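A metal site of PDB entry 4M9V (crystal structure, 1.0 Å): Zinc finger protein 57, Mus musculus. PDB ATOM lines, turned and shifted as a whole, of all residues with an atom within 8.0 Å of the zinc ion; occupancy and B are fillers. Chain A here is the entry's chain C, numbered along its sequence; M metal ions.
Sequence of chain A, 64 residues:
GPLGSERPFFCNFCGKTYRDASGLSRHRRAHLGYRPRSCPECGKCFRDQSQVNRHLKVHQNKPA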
ATOM      1  N   PHE A  10      -7.518   1.224 -11.622  1.00  0.00           N
ATOM      2  CA  PHE A  10      -8.772   1.600 -10.979  1.00  0.00           C
ATOM      3  C   PHE A  10      -8.683   1.693  -9.464  1.00  0.00           C
ATOM      4  O   PHE A  10      -7.835   1.076  -8.811  1.00  0.00           O
ATOM      5  CB  PHE A  10      -9.914   0.643 -11.380  1.00  0.00           C
ATOM      6  CG  PHE A  10      -9.775  -0.731 -10.819  1.00  0.00           C
ATOM      7  CD1 PHE A  10      -9.002  -1.674 -11.466  1.00  0.00           C
ATOM      8  CD2 PHE A  10     -10.428  -1.088  -9.654  1.00  0.00           C
ATOM      9  CE1 PHE A  10      -8.877  -2.933 -10.958  1.00  0.00           C
ATOM     10  CE2 PHE A  10     -10.305  -2.361  -9.136  1.00  0.00           C
ATOM     11  CZ  PHE A  10      -9.529  -3.277  -9.793  1.00  0.00           C
ATOM     12  N   CYS A  11      -9.609   2.481  -8.932  1.00  0.00           N
ATOM     13  CA  CYS A  11      -9.717   2.743  -7.520  1.00  0.00           C
ATOM     14  C   CYS A  11     -10.430   1.619  -6.785  1.00  0.00           C
ATOM     15  O   CYS A  11     -11.508   1.188  -7.212  1.00  0.00           O
ATOM     16  CB  CYS A  11     -10.508   4.032  -7.330  1.00  0.00           C
ATOM     17  SG  CYS A  11     -10.792   4.466  -5.619  1.00  0.00           S
ATOM     18  N   ASN A  12      -9.872   1.181  -5.659  1.00  0.00           N
ATOM     19  CA  ASN A  12     -10.467   0.101  -4.899  1.00  0.00           C
ATOM     20  C   ASN A  12     -11.580   0.544  -3.950  1.00  0.00           C
ATOM     21  O   ASN A  12     -12.194  -0.301  -3.296  1.00  0.00           O
ATOM     22  CB  ASN A  12      -9.385  -0.653  -4.102  1.00  0.00           C
ATOM     23  CG  ASN A  12      -8.365  -1.334  -4.992  1.00  0.00           C
ATOM     24  OD1 ASN A  12      -8.693  -1.852  -6.061  1.00  0.00           O
ATOM     25  ND2 ASN A  12      -7.113  -1.328  -4.549  1.00  0.00           N
ATOM     26  N   PHE A  13     -11.952   1.800  -3.940  1.00  0.00           N
ATOM     27  CA  PHE A  13     -13.092   2.123  -3.110  1.00  0.00           C
ATOM     28  C   PHE A  13     -14.267   2.609  -3.918  1.00  0.00           C
ATOM     29  O   PHE A  13     -15.399   2.572  -3.442  1.00  0.00           O
ATOM     30  CB  PHE A  13     -12.695   3.145  -2.076  1.00  0.00           C
ATOM     31  CG  PHE A  13     -11.633   2.665  -1.145  1.00  0.00           C
ATOM     32  CD1 PHE A  13     -10.301   2.768  -1.491  1.00  0.00           C
ATOM     33  CD2 PHE A  13     -11.961   2.110   0.080  1.00  0.00           C
ATOM     34  CE1 PHE A  13      -9.317   2.324  -0.634  1.00  0.00           C
ATOM     35  CE2 PHE A  13     -10.977   1.666   0.937  1.00  0.00           C
ATOM     36  CZ  PHE A  13      -9.658   1.784   0.580  1.00  0.00           C
ATOM     37  N   CYS A  14     -14.013   3.066  -5.144  1.00  0.00           N
ATOM     38  CA  CYS A  14     -15.158   3.485  -5.959  1.00  0.00           C
ATOM     39  C   CYS A  14     -15.095   3.042  -7.411  1.00  0.00           C
ATOM     40  O   CYS A  14     -16.014   3.338  -8.182  1.00  0.00           O
ATOM     41  CB  CYS A  14     -15.304   5.016  -5.922  1.00  0.00           C
ATOM     42  SG  CYS A  14     -14.162   5.912  -7.022  1.00  0.00           S
ATOM     43  N   GLY A  15     -14.031   2.348  -7.807  1.00  0.00           N
ATOM     44  CA  GLY A  15     -13.968   1.771  -9.126  1.00  0.00           C
ATOM     45  C   GLY A  15     -13.617   2.709 -10.266  1.00  0.00           C
ATOM     46  O   GLY A  15     -13.562   2.278 -11.408  1.00  0.00           O
ATOM     47  N   LYS A  16     -13.375   3.988  -9.985  1.00  0.00           N
ATOM     48  CA  LYS A  16     -13.044   4.900 -11.065  1.00  0.00           C
ATOM     49  C   LYS A  16     -11.775   4.444 -11.766  1.00  0.00           C
ATOM     50  O   LYS A  16     -10.807   4.013 -11.130  1.00  0.00           O
ATOM     51  CB  LYS A  16     -12.925   6.337 -10.553  1.00  0.00           C
ATOM     52  CG  LYS A  16     -14.246   7.088 -10.721  1.00  0.00           C
ATOM     53  CD  LYS A  16     -14.212   8.485 -10.151  1.00  0.00           C
ATOM     54  CE  LYS A  16     -13.144   9.309 -10.813  1.00  0.00           C
ATOM     55  NZ  LYS A  16     -13.426   9.579 -12.244  1.00  0.00           N
ATOM     56  N   THR A  17     -11.806   4.524 -13.090  1.00  0.00           N
ATOM     57  CA  THR A  17     -10.731   3.980 -13.929  1.00  0.00           C
ATOM     58  C   THR A  17      -9.871   5.076 -14.546  1.00  0.00           C
ATOM     59  O   THR A  17     -10.317   6.224 -14.707  1.00  0.00           O
ATOM     60  CB  THR A  17     -11.298   3.125 -15.065  1.00  0.00           C
ATOM     61  OG1 THR A  17     -12.001   3.972 -15.975  1.00  0.00           O
ATOM     62  CG2 THR A  17     -12.231   2.043 -14.522  1.00  0.00           C
ATOM     63  N   TYR A  18      -8.640   4.699 -14.899  1.00  0.00           N
ATOM     64  CA  TYR A  18      -7.608   5.607 -15.354  1.00  0.00           C
ATOM     65  C   TYR A  18      -6.784   4.987 -16.475  1.00  0.00           C
ATOM     66  O   TYR A  18      -6.570   3.769 -16.504  1.00  0.00           O
ATOM     67  CB  TYR A  18      -6.691   6.027 -14.184  1.00  0.00           C
ATOM     68  CG  TYR A  18      -7.481   6.884 -13.246  1.00  0.00           C
ATOM     69  CD1 TYR A  18      -7.701   8.219 -13.550  1.00  0.00           C
ATOM     70  CD2 TYR A  18      -8.150   6.342 -12.149  1.00  0.00           C
ATOM     71  CE1 TYR A  18      -8.513   8.998 -12.762  1.00  0.00           C
ATOM     72  CE2 TYR A  18      -8.956   7.113 -11.360  1.00  0.00           C
ATOM     73  CZ  TYR A  18      -9.147   8.445 -11.673  1.00  0.00           C
ATOM     74  OH  TYR A  18      -9.976   9.197 -10.885  1.00  0.00           O
ATOM     75  N   LEU A  24      -4.689   7.604 -11.208  1.00  0.00           N
ATOM     76  CA  LEU A  24      -5.082   6.813 -10.062  1.00  0.00           C
ATOM     77  C   LEU A  24      -4.371   7.278  -8.783  1.00  0.00           C
ATOM     78  O   LEU A  24      -4.989   7.391  -7.744  1.00  0.00           O
ATOM     79  CB  LEU A  24      -4.821   5.324 -10.315  1.00  0.00           C
ATOM     80  CG  LEU A  24      -5.128   4.410  -9.133  1.00  0.00           C
ATOM     81  CD1 LEU A  24      -6.608   4.502  -8.697  1.00  0.00           C
ATOM     82  CD2 LEU A  24      -4.759   2.966  -9.471  1.00  0.00           C
ATOM     83  N   HIS A  27      -6.095  10.411  -7.699  1.00  0.00           N
ATOM     84  CA  HIS A  27      -7.444  10.120  -7.250  1.00  0.00           C
ATOM     85  C   HIS A  27      -7.432   9.502  -5.857  1.00  0.00           C
ATOM     86  O   HIS A  27      -8.205   9.893  -4.971  1.00  0.00           O
ATOM     87  CB  HIS A  27      -8.123   9.206  -8.270  1.00  0.00           C
ATOM     88  CG  HIS A  27      -9.465   8.715  -7.828  1.00  0.00           C
ATOM     89  ND1 HIS A  27     -10.611   9.469  -7.937  1.00  0.00           N
ATOM     90  CD2 HIS A  27      -9.832   7.537  -7.275  1.00  0.00           C
ATOM     91  CE1 HIS A  27     -11.636   8.759  -7.485  1.00  0.00           C
ATOM     92  NE2 HIS A  27     -11.190   7.585  -7.083  1.00  0.00           N
ATOM     93  N   ARG A  28      -6.573   8.509  -5.638  1.00  0.00           N
ATOM     94  CA  ARG A  28      -6.452   7.871  -4.330  1.00  0.00           C
ATOM     95  C   ARG A  28      -6.113   8.899  -3.259  1.00  0.00           C
ATOM     96  O   ARG A  28      -6.679   8.915  -2.175  1.00  0.00           O
ATOM     97  CB  ARG A  28      -5.371   6.788  -4.318  1.00  0.00           C
ATOM     98  CG  ARG A  28      -5.616   5.568  -5.141  1.00  0.00           C
ATOM     99  CD  ARG A  28      -4.442   4.555  -4.996  1.00  0.00           C
ATOM    100  NE  ARG A  28      -3.115   5.136  -5.230  1.00  0.00           N
ATOM    101  CZ  ARG A  28      -2.168   4.570  -5.995  1.00  0.00           C
ATOM    102  NH1 ARG A  28      -0.977   5.174  -6.157  1.00  0.00           N
ATOM    103  NH2 ARG A  28      -2.401   3.422  -6.608  1.00  0.00           N
ATOM    104  N   ALA A  30      -6.664  12.051  -3.339  1.00  0.00           N
ATOM    105  CA  ALA A  30      -7.811  12.937  -3.150  1.00  0.00           C
ATOM    106  C   ALA A  30      -8.817  12.309  -2.178  1.00  0.00           C
ATOM    107  O   ALA A  30      -9.311  12.991  -1.272  1.00  0.00           O
ATOM    108  CB  ALA A  30      -8.458  13.304  -4.480  1.00  0.00           C
ATOM    109  N   HIS A  31      -9.091  11.014  -2.300  1.00  0.00           N
ATOM    110  CA  HIS A  31      -9.932  10.354  -1.289  1.00  0.00           C
ATOM    111  C   HIS A  31      -9.312  10.496   0.101  1.00  0.00           C
ATOM    112  O   HIS A  31     -10.035  10.663   1.084  1.00  0.00           O
ATOM    113  CB  HIS A  31     -10.094   8.847  -1.532  1.00  0.00           C
ATOM    114  CG  HIS A  31     -11.067   8.427  -2.605  1.00  0.00           C
ATOM    115  ND1 HIS A  31     -12.417   8.728  -2.586  1.00  0.00           N
ATOM    116  CD2 HIS A  31     -10.891   7.571  -3.643  1.00  0.00           C
ATOM    117  CE1 HIS A  31     -13.012   8.125  -3.607  1.00  0.00           C
ATOM    118  NE2 HIS A  31     -12.115   7.410  -4.262  1.00  0.00           N
HETATM  119 ZN    ZN M   1     -12.216   6.257  -5.930  1.00  0.00          ZN
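The side-chain hydroxyl (OH) of Tyr 18 lies within hydrogen-bond range of a ring nitrogen (ND1) of His 27 (3.0 Å). SG of Cys 14 lies close to N of Lys 16 (3.6 Å). N of Phe 13 lies close to SG of Cys 11 (3.4 Å). N of Cys 11 lies within hydrogen-bond range of O of Lys 16, 2.9 Å away.
The zinc ion is bound by a ring nitrogen (NE2) of His 31 (2.0 Å), a ring nitrogen (NE2) of His 27 (2.0 Å), the side-chain sulfur (SG) of Cys 14 (2.3 Å) and the side-chain sulfur (SG) of Cys 11 (2.3 Å).
Within 4 Å of the zinc ion: Cys 11, Cys 14, His 27 and His 31. The nearest printed residue that does not touch the zinc ion is Phe 13 (4.6 Å).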
